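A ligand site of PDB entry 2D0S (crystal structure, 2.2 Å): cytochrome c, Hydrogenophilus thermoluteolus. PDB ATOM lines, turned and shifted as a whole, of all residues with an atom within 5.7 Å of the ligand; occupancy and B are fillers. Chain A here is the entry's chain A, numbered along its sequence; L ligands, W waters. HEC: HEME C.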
ATOM      1  N   ALA A   5      -6.337  -0.361 -20.168  1.00  0.00           N
ATOM      2  CA  ALA A   5      -5.024  -0.361 -20.769  1.00  0.00           C
ATOM      3  C   ALA A   5      -4.099  -1.195 -19.919  1.00  0.00           C
ATOM      4  O   ALA A   5      -3.347  -2.065 -20.415  1.00  0.00           O
ATOM      5  CB  ALA A   5      -4.482   1.087 -20.887  1.00  0.00           C
ATOM      6  N   LYS A   8      -4.813  -4.892 -19.931  1.00  0.00           N
ATOM      7  CA  LYS A   8      -4.366  -5.581 -21.154  1.00  0.00           C
ATOM      8  C   LYS A   8      -2.864  -5.602 -21.372  1.00  0.00           C
ATOM      9  O   LYS A   8      -2.418  -5.948 -22.466  1.00  0.00           O
ATOM     10  CB  LYS A   8      -5.125  -5.133 -22.392  1.00  0.00           C
ATOM     11  CG  LYS A   8      -6.625  -5.296 -22.313  1.00  0.00           C
ATOM     12  CD  LYS A   8      -6.970  -6.699 -22.056  1.00  0.00           C
ATOM     13  CE  LYS A   8      -8.439  -6.854 -21.698  1.00  0.00           C
ATOM     14  NZ  LYS A   8      -8.802  -8.296 -21.917  1.00  0.00           N
ATOM     15  N   GLY A   9      -2.115  -5.282 -20.321  1.00  0.00           N
ATOM     16  CA  GLY A   9      -0.647  -5.320 -20.366  1.00  0.00           C
ATOM     17  C   GLY A   9       0.111  -4.172 -21.008  1.00  0.00           C
ATOM     18  O   GLY A   9       1.354  -4.202 -21.097  1.00  0.00           O
ATOM     19  N   CYS A  10      -0.654  -3.208 -21.504  1.00  0.00           N
ATOM     20  CA  CYS A  10      -0.117  -2.071 -22.181  1.00  0.00           C
ATOM     21  C   CYS A  10       0.884  -1.284 -21.440  1.00  0.00           C
ATOM     22  O   CYS A  10       1.812  -0.725 -22.063  1.00  0.00           O
ATOM     23  CB  CYS A  10      -1.246  -1.136 -22.593  1.00  0.00           C
ATOM     24  SG  CYS A  10      -2.539  -1.905 -23.564  1.00  0.00           S
ATOM     25  N   ALA A  12       3.099  -1.958 -19.401  1.00  0.00           N
ATOM     26  CA  ALA A  12       4.402  -2.511 -19.166  1.00  0.00           C
ATOM     27  C   ALA A  12       5.335  -1.710 -20.038  1.00  0.00           C
ATOM     28  O   ALA A  12       6.485  -1.523 -19.687  1.00  0.00           O
ATOM     29  CB  ALA A  12       4.465  -4.001 -19.555  1.00  0.00           C
ATOM     30  N   CYS A  13       4.864  -1.379 -21.251  1.00  0.00           N
ATOM     31  CA  CYS A  13       5.745  -0.775 -22.256  1.00  0.00           C
ATOM     32  C   CYS A  13       5.495   0.706 -22.519  1.00  0.00           C
ATOM     33  O   CYS A  13       6.187   1.306 -23.302  1.00  0.00           O
ATOM     34  CB  CYS A  13       5.562  -1.536 -23.549  1.00  0.00           C
ATOM     35  SG  CYS A  13       6.205  -3.229 -23.760  1.00  0.00           S
ATOM     36  N   HIS A  14       4.404   1.245 -21.950  1.00  0.00           N
ATOM     37  CA  HIS A  14       3.954   2.605 -22.237  1.00  0.00           C
ATOM     38  C   HIS A  14       3.554   3.223 -20.915  1.00  0.00           C
ATOM     39  O   HIS A  14       2.865   2.590 -20.119  1.00  0.00           O
ATOM     40  CB  HIS A  14       2.684   2.625 -23.142  1.00  0.00           C
ATOM     41  CG  HIS A  14       2.893   2.157 -24.543  1.00  0.00           C
ATOM     42  ND1 HIS A  14       3.429   2.965 -25.524  1.00  0.00           N
ATOM     43  CD2 HIS A  14       2.496   1.012 -25.168  1.00  0.00           C
ATOM     44  CE1 HIS A  14       3.415   2.309 -26.687  1.00  0.00           C
ATOM     45  NE2 HIS A  14       2.879   1.113 -26.495  1.00  0.00           N
ATOM     46  N   VAL A  21       9.719   1.337 -23.136  1.00  0.00           N
ATOM     47  CA  VAL A  21       9.971   0.744 -24.444  1.00  0.00           C
ATOM     48  C   VAL A  21       9.238   1.512 -25.625  1.00  0.00           C
ATOM     49  O   VAL A  21       9.807   1.693 -26.727  1.00  0.00           O
ATOM     50  CB  VAL A  21       9.566  -0.710 -24.451  1.00  0.00           C
ATOM     51  CG1 VAL A  21      10.202  -1.430 -25.592  1.00  0.00           C
ATOM     52  CG2 VAL A  21       9.955  -1.356 -23.106  1.00  0.00           C
ATOM     53  N   GLY A  22       7.945   1.808 -25.432  1.00  0.00           N
ATOM     54  CA  GLY A  22       7.173   2.435 -26.501  1.00  0.00           C
ATOM     55  C   GLY A  22       6.984   3.869 -26.141  1.00  0.00           C
ATOM     56  O   GLY A  22       7.344   4.304 -24.984  1.00  0.00           O
ATOM     57  N   PRO A  23       6.402   4.651 -27.078  1.00  0.00           N
ATOM     58  CA  PRO A  23       6.205   6.070 -26.794  1.00  0.00           C
ATOM     59  C   PRO A  23       5.223   6.281 -25.634  1.00  0.00           C
ATOM     60  O   PRO A  23       4.309   5.455 -25.397  1.00  0.00           O
ATOM     61  CB  PRO A  23       5.639   6.612 -28.126  1.00  0.00           C
ATOM     62  CG  PRO A  23       4.990   5.414 -28.762  1.00  0.00           C
ATOM     63  CD  PRO A  23       5.955   4.293 -28.428  1.00  0.00           C
ATOM     64  N   TYR A  25       2.001   7.909 -24.001  1.00  0.00           N
ATOM     65  CA  TYR A  25       0.667   8.105 -24.542  1.00  0.00           C
ATOM     66  C   TYR A  25       0.445   9.575 -24.858  1.00  0.00           C
ATOM     67  O   TYR A  25      -0.266   9.892 -25.753  1.00  0.00           O
ATOM     68  CB  TYR A  25      -0.384   7.611 -23.550  1.00  0.00           C
ATOM     69  CG  TYR A  25      -0.484   6.106 -23.502  1.00  0.00           C
ATOM     70  CD1 TYR A  25      -0.716   5.458 -22.314  1.00  0.00           C
ATOM     71  CD2 TYR A  25      -0.268   5.336 -24.650  1.00  0.00           C
ATOM     72  CE1 TYR A  25      -0.774   4.098 -22.243  1.00  0.00           C
ATOM     73  CE2 TYR A  25      -0.403   3.957 -24.614  1.00  0.00           C
ATOM     74  CZ  TYR A  25      -0.655   3.358 -23.394  1.00  0.00           C
ATOM     75  OH  TYR A  25      -0.739   2.009 -23.292  1.00  0.00           O
ATOM     76  N   VAL A  28       1.801  10.087 -28.233  1.00  0.00           N
ATOM     77  CA  VAL A  28       0.897   9.462 -29.218  1.00  0.00           C
ATOM     78  C   VAL A  28      -0.234  10.447 -29.467  1.00  0.00           C
ATOM     79  O   VAL A  28      -0.498  10.771 -30.610  1.00  0.00           O
ATOM     80  CB  VAL A  28       0.352   8.070 -28.794  1.00  0.00           C
ATOM     81  CG1 VAL A  28      -0.827   7.604 -29.780  1.00  0.00           C
ATOM     82  CG2 VAL A  28       1.511   6.998 -28.796  1.00  0.00           C
ATOM     83  N   LYS A  31       0.896  13.248 -31.732  1.00  0.00           N
ATOM     84  CA  LYS A  31       1.132  12.923 -33.093  1.00  0.00           C
ATOM     85  C   LYS A  31      -0.169  12.663 -33.881  1.00  0.00           C
ATOM     86  O   LYS A  31      -0.215  12.904 -35.059  1.00  0.00           O
ATOM     87  CB  LYS A  31       2.065  11.731 -33.174  1.00  0.00           C
ATOM     88  CG  LYS A  31       2.738  11.584 -34.518  1.00  0.00           C
ATOM     89  CD  LYS A  31       4.012  10.745 -34.376  1.00  0.00           C
ATOM     90  CE  LYS A  31       4.427  10.098 -35.716  1.00  0.00           C
ATOM     91  NZ  LYS A  31       3.265   9.423 -36.456  1.00  0.00           N
ATOM     92  N   TYR A  32      -1.202  12.141 -33.220  1.00  0.00           N
ATOM     93  CA  TYR A  32      -2.406  11.745 -33.959  1.00  0.00           C
ATOM     94  C   TYR A  32      -3.623  12.515 -33.528  1.00  0.00           C
ATOM     95  O   TYR A  32      -3.594  13.190 -32.467  1.00  0.00           O
ATOM     96  CB  TYR A  32      -2.669  10.260 -33.801  1.00  0.00           C
ATOM     97  CG  TYR A  32      -1.524   9.423 -34.259  1.00  0.00           C
ATOM     98  CD1 TYR A  32      -1.322   9.177 -35.614  1.00  0.00           C
ATOM     99  CD2 TYR A  32      -0.599   8.920 -33.342  1.00  0.00           C
ATOM    100  CE1 TYR A  32      -0.262   8.414 -36.051  1.00  0.00           C
ATOM    101  CE2 TYR A  32       0.468   8.120 -33.775  1.00  0.00           C
ATOM    102  CZ  TYR A  32       0.624   7.880 -35.127  1.00  0.00           C
ATOM    103  OH  TYR A  32       1.643   7.072 -35.554  1.00  0.00           O
ATOM    104  N   LEU A  40      -4.474   3.225 -35.897  1.00  0.00           N
ATOM    105  CA  LEU A  40      -3.801   2.838 -34.655  1.00  0.00           C
ATOM    106  C   LEU A  40      -4.255   1.490 -34.133  1.00  0.00           C
ATOM    107  O   LEU A  40      -3.454   0.720 -33.577  1.00  0.00           O
ATOM    108  CB  LEU A  40      -4.002   3.917 -33.561  1.00  0.00           C
ATOM    109  CG  LEU A  40      -3.346   5.217 -33.934  1.00  0.00           C
ATOM    110  CD1 LEU A  40      -3.672   6.301 -32.912  1.00  0.00           C
ATOM    111  CD2 LEU A  40      -1.871   4.982 -34.011  1.00  0.00           C
ATOM    112  N   LYS A  43      -2.478  -1.220 -35.936  1.00  0.00           N
ATOM    113  CA  LYS A  43      -1.097  -1.244 -35.447  1.00  0.00           C
ATOM    114  C   LYS A  43      -0.964  -2.027 -34.096  1.00  0.00           C
ATOM    115  O   LYS A  43      -0.026  -2.776 -33.888  1.00  0.00           O
ATOM    116  CB  LYS A  43      -0.567   0.200 -35.311  1.00  0.00           C
ATOM    117  CG  LYS A  43       0.856   0.333 -34.780  1.00  0.00           C
ATOM    118  CD  LYS A  43       1.875  -0.448 -35.631  1.00  0.00           C
ATOM    119  CE  LYS A  43       3.302  -0.201 -35.138  1.00  0.00           C
ATOM    120  NZ  LYS A  43       3.839   1.171 -35.581  1.00  0.00           N
ATOM    121  N   VAL A  44      -1.897  -1.839 -33.190  1.00  0.00           N
ATOM    122  CA  VAL A  44      -1.831  -2.502 -31.906  1.00  0.00           C
ATOM    123  C   VAL A  44      -2.098  -4.000 -32.160  1.00  0.00           C
ATOM    124  O   VAL A  44      -1.361  -4.874 -31.671  1.00  0.00           O
ATOM    125  CB  VAL A  44      -2.861  -1.938 -30.918  1.00  0.00           C
ATOM    126  CG1 VAL A  44      -2.837  -2.720 -29.598  1.00  0.00           C
ATOM    127  CG2 VAL A  44      -2.623  -0.406 -30.710  1.00  0.00           C
ATOM    128  N   GLY A  48       4.144  -4.169 -34.858  1.00  0.00           N
ATOM    129  CA  GLY A  48       5.052  -3.595 -35.854  1.00  0.00           C
ATOM    130  C   GLY A  48       6.021  -2.539 -35.339  1.00  0.00           C
ATOM    131  O   GLY A  48       5.989  -2.172 -34.163  1.00  0.00           O
ATOM    132  N   ALA A  49       6.892  -2.092 -36.250  1.00  0.00           N
ATOM    133  CA  ALA A  49       7.952  -1.154 -35.874  1.00  0.00           C
ATOM    134  C   ALA A  49       8.033   0.049 -36.826  1.00  0.00           C
ATOM    135  O   ALA A  49       7.351   0.080 -37.848  1.00  0.00           O
ATOM    136  CB  ALA A  49       9.250  -1.947 -35.918  1.00  0.00           C
ATOM    137  N   GLY A  50       9.049   0.865 -36.548  1.00  0.00           N
ATOM    138  CA  GLY A  50       9.473   1.930 -37.424  1.00  0.00           C
ATOM    139  C   GLY A  50       8.963   3.347 -37.371  1.00  0.00           C
ATOM    140  O   GLY A  50       9.616   4.288 -37.825  1.00  0.00           O
ATOM    141  N   VAL A  51       7.797   3.527 -36.787  1.00  0.00           N
ATOM    142  CA  VAL A  51       7.283   4.881 -36.624  1.00  0.00           C
ATOM    143  C   VAL A  51       8.046   5.669 -35.569  1.00  0.00           C
ATOM    144  O   VAL A  51       8.326   6.844 -35.762  1.00  0.00           O
ATOM    145  CB  VAL A  51       5.792   4.857 -36.353  1.00  0.00           C
ATOM    146  CG1 VAL A  51       5.278   6.241 -36.189  1.00  0.00           C
ATOM    147  CG2 VAL A  51       5.073   4.116 -37.485  1.00  0.00           C
ATOM    148  N   TRP A  52       8.369   5.019 -34.450  1.00  0.00           N
ATOM    149  CA  TRP A  52       9.076   5.657 -33.343  1.00  0.00           C
ATOM    150  C   TRP A  52      10.504   5.104 -33.139  1.00  0.00           C
ATOM    151  O   TRP A  52      11.236   5.585 -32.271  1.00  0.00           O
ATOM    152  CB  TRP A  52       8.247   5.405 -32.068  1.00  0.00           C
ATOM    153  CG  TRP A  52       6.841   5.999 -32.131  1.00  0.00           C
ATOM    154  CD1 TRP A  52       5.738   5.406 -32.607  1.00  0.00           C
ATOM    155  CD2 TRP A  52       6.426   7.318 -31.683  1.00  0.00           C
ATOM    156  NE1 TRP A  52       4.638   6.245 -32.470  1.00  0.00           N
ATOM    157  CE2 TRP A  52       5.036   7.404 -31.849  1.00  0.00           C
ATOM    158  CE3 TRP A  52       7.095   8.407 -31.058  1.00  0.00           C
ATOM    159  CZ2 TRP A  52       4.304   8.572 -31.537  1.00  0.00           C
ATOM    160  CZ3 TRP A  52       6.358   9.534 -30.712  1.00  0.00           C
ATOM    161  CH2 TRP A  52       4.981   9.613 -30.971  1.00  0.00           C
ATOM    162  N   GLY A  53      10.828   4.015 -33.834  1.00  0.00           N
ATOM    163  CA  GLY A  53      12.104   3.357 -33.585  1.00  0.00           C
ATOM    164  C   GLY A  53      12.134   1.993 -34.209  1.00  0.00           C
ATOM    165  O   GLY A  53      11.166   1.574 -34.873  1.00  0.00           O
ATOM    166  N   PRO A  54      13.240   1.254 -33.986  1.00  0.00           N
ATOM    167  CA  PRO A  54      13.398  -0.075 -34.573  1.00  0.00           C
ATOM    168  C   PRO A  54      12.804  -1.233 -33.764  1.00  0.00           C
ATOM    169  O   PRO A  54      12.767  -2.346 -34.264  1.00  0.00           O
ATOM    170  CB  PRO A  54      14.917  -0.226 -34.628  1.00  0.00           C
ATOM    171  CG  PRO A  54      15.399   0.527 -33.388  1.00  0.00           C
ATOM    172  CD  PRO A  54      14.450   1.704 -33.263  1.00  0.00           C
ATOM    173  N   VAL A  55      12.458  -1.006 -32.491  1.00  0.00           N
ATOM    174  CA  VAL A  55      11.882  -2.111 -31.671  1.00  0.00           C
ATOM    175  C   VAL A  55      10.367  -2.284 -31.874  1.00  0.00           C
ATOM    176  O   VAL A  55       9.624  -1.307 -31.828  1.00  0.00           O
ATOM    177  CB  VAL A  55      12.289  -2.027 -30.164  1.00  0.00           C
ATOM    178  CG1 VAL A  55      12.584  -0.599 -29.763  1.00  0.00           C
ATOM    179  CG2 VAL A  55      11.233  -2.643 -29.255  1.00  0.00           C
ATOM    180  N   PRO A  56       9.931  -3.489 -32.292  1.00  0.00           N
ATOM    181  CA  PRO A  56       8.555  -3.742 -32.640  1.00  0.00           C
ATOM    182  C   PRO A  56       7.656  -3.875 -31.387  1.00  0.00           C
ATOM    183  O   PRO A  56       8.103  -4.316 -30.325  1.00  0.00           O
ATOM    184  CB  PRO A  56       8.640  -5.069 -33.413  1.00  0.00           C
ATOM    185  CG  PRO A  56       9.792  -5.760 -32.851  1.00  0.00           C
ATOM    186  CD  PRO A  56      10.776  -4.697 -32.480  1.00  0.00           C
ATOM    187  N   MET A  57       6.401  -3.534 -31.599  1.00  0.00           N
ATOM    188  CA  MET A  57       5.387  -3.630 -30.605  1.00  0.00           C
ATOM    189  C   MET A  57       4.866  -4.990 -31.070  1.00  0.00           C
ATOM    190  O   MET A  57       4.558  -5.155 -32.276  1.00  0.00           O
ATOM    191  CB  MET A  57       4.253  -2.580 -30.687  1.00  0.00           C
ATOM    192  CG  MET A  57       2.919  -3.060 -30.009  1.00  0.00           C
ATOM    193  SD  MET A  57       1.701  -1.758 -29.636  1.00  0.00           S
ATOM    194  CE  MET A  57       1.623  -0.871 -31.237  1.00  0.00           C
ATOM    195  N   PRO A  58       4.717  -5.944 -30.128  1.00  0.00           N
ATOM    196  CA  PRO A  58       4.144  -7.240 -30.499  1.00  0.00           C
ATOM    197  C   PRO A  58       2.658  -7.167 -30.910  1.00  0.00           C
ATOM    198  O   PRO A  58       1.938  -6.220 -30.541  1.00  0.00           O
ATOM    199  CB  PRO A  58       4.348  -8.092 -29.255  1.00  0.00           C
ATOM    200  CG  PRO A  58       4.534  -7.091 -28.122  1.00  0.00           C
ATOM    201  CD  PRO A  58       5.038  -5.837 -28.694  1.00  0.00           C
ATOM    202  N   HIS A  60      -1.341  -8.217 -30.917  1.00  0.00           N
ATOM    203  CA  HIS A  60      -2.248  -8.593 -29.832  1.00  0.00           C
ATOM    204  C   HIS A  60      -3.387  -9.392 -30.386  1.00  0.00           C
ATOM    205  O   HIS A  60      -4.485  -8.890 -30.481  1.00  0.00           O
ATOM    206  CB  HIS A  60      -2.774  -7.363 -29.126  1.00  0.00           C
ATOM    207  CG  HIS A  60      -1.710  -6.566 -28.432  1.00  0.00           C
ATOM    208  ND1 HIS A  60      -1.416  -6.731 -27.096  1.00  0.00           N
ATOM    209  CD2 HIS A  60      -0.850  -5.639 -28.892  1.00  0.00           C
ATOM    210  CE1 HIS A  60      -0.438  -5.908 -26.757  1.00  0.00           C
ATOM    211  NE2 HIS A  60      -0.050  -5.258 -27.841  1.00  0.00           N
ATOM    212  N   VAL A  63      -6.650  -9.925 -27.887  1.00  0.00           N
ATOM    213  CA  VAL A  63      -7.325  -8.798 -27.203  1.00  0.00           C
ATOM    214  C   VAL A  63      -8.372  -8.324 -28.156  1.00  0.00           C
ATOM    215  O   VAL A  63      -8.111  -8.218 -29.361  1.00  0.00           O
ATOM    216  CB  VAL A  63      -6.306  -7.640 -26.828  1.00  0.00           C
ATOM    217  CG1 VAL A  63      -7.026  -6.438 -26.107  1.00  0.00           C
ATOM    218  CG2 VAL A  63      -5.199  -8.188 -25.950  1.00  0.00           C
ATOM    219  N   ILE A  68      -9.287  -2.804 -27.724  1.00  0.00           N
ATOM    220  CA  ILE A  68      -8.209  -2.017 -28.256  1.00  0.00           C
ATOM    221  C   ILE A  68      -8.723  -0.613 -28.637  1.00  0.00           C
ATOM    222  O   ILE A  68      -8.118   0.387 -28.277  1.00  0.00           O
ATOM    223  CB  ILE A  68      -7.549  -2.684 -29.484  1.00  0.00           C
ATOM    224  CG1 ILE A  68      -6.856  -3.975 -29.061  1.00  0.00           C
ATOM    225  CG2 ILE A  68      -6.544  -1.727 -30.090  1.00  0.00           C
ATOM    226  CD1 ILE A  68      -6.349  -4.804 -30.236  1.00  0.00           C
ATOM    227  N   ILE A  71      -9.141   1.678 -25.726  1.00  0.00           N
ATOM    228  CA  ILE A  71      -7.905   2.164 -25.118  1.00  0.00           C
ATOM    229  C   ILE A  71      -7.374   3.280 -26.015  1.00  0.00           C
ATOM    230  O   ILE A  71      -7.099   4.389 -25.547  1.00  0.00           O
ATOM    231  CB  ILE A  71      -6.868   1.065 -24.955  1.00  0.00           C
ATOM    232  CG1 ILE A  71      -7.368  -0.002 -23.939  1.00  0.00           C
ATOM    233  CG2 ILE A  71      -5.448   1.691 -24.538  1.00  0.00           C
ATOM    234  CD1 ILE A  71      -6.602  -1.438 -24.068  1.00  0.00           C
ATOM    235  N   VAL A  72      -7.438   3.066 -27.325  1.00  0.00           N
ATOM    236  CA  VAL A  72      -6.901   4.016 -28.253  1.00  0.00           C
ATOM    237  C   VAL A  72      -7.638   5.368 -28.219  1.00  0.00           C
ATOM    238  O   VAL A  72      -7.007   6.433 -28.174  1.00  0.00           O
ATOM    239  CB  VAL A  72      -6.792   3.450 -29.669  1.00  0.00           C
ATOM    240  CG1 VAL A  72      -6.638   4.578 -30.669  1.00  0.00           C
ATOM    241  CG2 VAL A  72      -5.549   2.456 -29.778  1.00  0.00           C
ATOM    242  N   VAL A  75      -6.308   7.077 -24.971  1.00  0.00           N
ATOM    243  CA  VAL A  75      -4.982   7.627 -25.249  1.00  0.00           C
ATOM    244  C   VAL A  75      -5.056   8.993 -25.934  1.00  0.00           C
ATOM    245  O   VAL A  75      -4.340   9.945 -25.548  1.00  0.00           O
ATOM    246  CB  VAL A  75      -4.142   6.671 -26.097  1.00  0.00           C
ATOM    247  CG1 VAL A  75      -2.868   7.384 -26.664  1.00  0.00           C
ATOM    248  CG2 VAL A  75      -3.744   5.464 -25.276  1.00  0.00           C
HETATM  249 FE   HEC L   1       2.390  -0.236 -27.894  1.00  0.00          FE
HETATM  250  CHA HEC L   1       3.583   1.826 -30.377  1.00  0.00           C
HETATM  251  CHB HEC L   1      -0.606   1.318 -27.947  1.00  0.00           C
HETATM  252  CHC HEC L   1       1.159  -2.681 -25.856  1.00  0.00           C
HETATM  253  CHD HEC L   1       5.605  -1.451 -27.413  1.00  0.00           C
HETATM  254  NA  HEC L   1       1.652   1.258 -28.909  1.00  0.00           N
HETATM  255  C1A HEC L   1       2.295   2.012 -29.909  1.00  0.00           C
HETATM  256  C2A HEC L   1       1.374   2.995 -30.415  1.00  0.00           C
HETATM  257  C3A HEC L   1       0.223   2.903 -29.721  1.00  0.00           C
HETATM  258  C4A HEC L   1       0.365   1.786 -28.781  1.00  0.00           C
HETATM  259  CMA HEC L   1      -1.072   3.752 -29.908  1.00  0.00           C
HETATM  260  CAA HEC L   1       1.718   4.044 -31.518  1.00  0.00           C
HETATM  261  CBA HEC L   1       1.516   3.352 -32.863  1.00  0.00           C
HETATM  262  CGA HEC L   1       2.103   4.144 -33.999  1.00  0.00           C
HETATM  263  O1A HEC L   1       2.390   5.348 -33.828  1.00  0.00           O
HETATM  264  O2A HEC L   1       2.250   3.561 -35.091  1.00  0.00           O
HETATM  265  NB  HEC L   1       0.622  -0.644 -27.069  1.00  0.00           N
HETATM  266  C1B HEC L   1      -0.514   0.122 -27.235  1.00  0.00           C
HETATM  267  C2B HEC L   1      -1.613  -0.561 -26.612  1.00  0.00           C
HETATM  268  C3B HEC L   1      -1.127  -1.657 -26.008  1.00  0.00           C
HETATM  269  C4B HEC L   1       0.279  -1.744 -26.331  1.00  0.00           C
HETATM  270  CMB HEC L   1      -3.032   0.052 -26.519  1.00  0.00           C
HETATM  271  CAB HEC L   1      -1.875  -2.688 -25.099  1.00  0.00           C
HETATM  272  CBB HEC L   1      -3.092  -3.305 -25.813  1.00  0.00           C
HETATM  273  NC  HEC L   1       3.221  -1.728 -26.845  1.00  0.00           N
HETATM  274  C1C HEC L   1       2.518  -2.639 -26.038  1.00  0.00           C
HETATM  275  C2C HEC L   1       3.475  -3.495 -25.371  1.00  0.00           C
HETATM  276  C3C HEC L   1       4.682  -3.280 -25.962  1.00  0.00           C
HETATM  277  C4C HEC L   1       4.547  -2.090 -26.778  1.00  0.00           C
HETATM  278  CMC HEC L   1       3.009  -4.759 -24.601  1.00  0.00           C
HETATM  279  CAC HEC L   1       6.109  -3.882 -25.651  1.00  0.00           C
HETATM  280  CBC HEC L   1       6.203  -5.355 -25.215  1.00  0.00           C
HETATM  281  ND  HEC L   1       4.344   0.112 -28.807  1.00  0.00           N
HETATM  282  C1D HEC L   1       5.505  -0.561 -28.450  1.00  0.00           C
HETATM  283  C2D HEC L   1       6.583  -0.077 -29.272  1.00  0.00           C
HETATM  284  C3D HEC L   1       5.955   0.969 -30.159  1.00  0.00           C
HETATM  285  C4D HEC L   1       4.565   1.022 -29.797  1.00  0.00           C
HETATM  286  CMD HEC L   1       8.046  -0.555 -29.226  1.00  0.00           C
HETATM  287  CAD HEC L   1       6.608   1.750 -31.289  1.00  0.00           C
HETATM  288  CBD HEC L   1       6.286   1.006 -32.572  1.00  0.00           C
HETATM  289  CGD HEC L   1       6.914   1.800 -33.716  1.00  0.00           C
HETATM  290  O1D HEC L   1       8.030   2.323 -33.492  1.00  0.00           O
HETATM  291  O2D HEC L   1       6.287   1.894 -34.829  1.00  0.00           O
HETATM  292  O   HOH W   1      10.047   1.388 -31.642  1.00  0.00           O
HETATM  293  O   HOH W   2      -0.107  -5.866 -24.018  1.00  0.00           O
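An oxygen (O1D) of the ligand sits at hydrogen-bond distance from the backbone NH (N) of Trp 52, 2.9 Å away.
An oxygen (O2D) of the ligand is in hydrogen-bond range of the backbone NH (N) of Val 51 (3.0 Å).
O2D of the ligand is in hydrogen-bond range of N of Gly 50 (3.4 Å).
The side-chain amino group of Lys 43 is in salt-bridge range of an oxygen (O2D) of the ligand (2.7 Å).
SD of Met 57 is bound to FE of the ligand.
NE2 of His 14 binds FE of the ligand, at 2.0 Å.
SG of Cys 13 is covalently linked to CAC of the ligand (2.0 Å).
An oxygen (O1A) of the ligand sits at hydrogen-bond distance from the indole nitrogen of Trp 52 (2.8 Å).
SG of Cys 10 is covalently linked to CAB of the ligand (1.8 Å).
An oxygen (O1A) of the ligand is in hydrogen-bond range of the side-chain hydroxyl of Tyr 32, 2.6 Å away.
O1D of the ligand is in hydrogen-bond range of N of Gly 53.
A ring nitrogen (ND1) of His 14 lies within hydrogen-bond range of the backbone carbonyl oxygen (O) of Pro 23, 2.6 Å away.
A ring nitrogen (NE2) of His 60 sits close to the backbone carbonyl oxygen (O) of Pro 58 (3.5 Å).
The backbone NH (N) of Gly 48 is in hydrogen-bond range of the backbone carbonyl oxygen (O) of Met 57.
N of His 60 sits close to O of Val 44 (3.4 Å).
The side-chain hydroxyl (OH) of Tyr 32 sits at hydrogen-bond distance from the side-chain amino group (NZ) of Lys 31.
The backbone carbonyl oxygen (O) of Ala 5 is in hydrogen-bond range of the backbone NH (N) of Cys 10.
The backbone carbonyl oxygen (O) of Cys 13 is in hydrogen-bond range of the backbone NH (N) of Gly 22, 2.8 Å away.
Gly 9 touches the ligand.
Val 21 touches the ligand (O to CMD, 3.8 Å).
Gly 22 touches the ligand.
Pro 23 touches the ligand.
CG1 of Val 28 touches CMA of the ligand (3.9 Å).
CD2 of Leu 40 touches CBA of the ligand (3.9 Å).
Val 44 touches the ligand.
O of Gly 48 touches CBD of the ligand, at 3.6 Å.
Ala 49 touches the ligand.
Val 55 touches the ligand.
Pro 56 touches the ligand.
Pro 58 touches the ligand (CD to CBC, 3.7 Å).
NE2 of His 60 touches CHC of the ligand, 3.5 Å away.
CG2 of Ile 71 touches CMB of the ligand, at 3.5 Å.
Of the 34 residues printed, 24 come within 4 Å of the ligand.
The nearest printed residue that does not touch the ligand is Lys 8 (4.2 Å).
Water W1 lies within hydrogen-bond range of O of Val 55 (2.7 Å), O1D of the ligand (2.9 Å) and O of Gly 53 (3.4 Å).
Water W2 lies within hydrogen-bond range of O of Lys 8 (2.8 Å) and ND1 of His 60 (3.5 Å).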
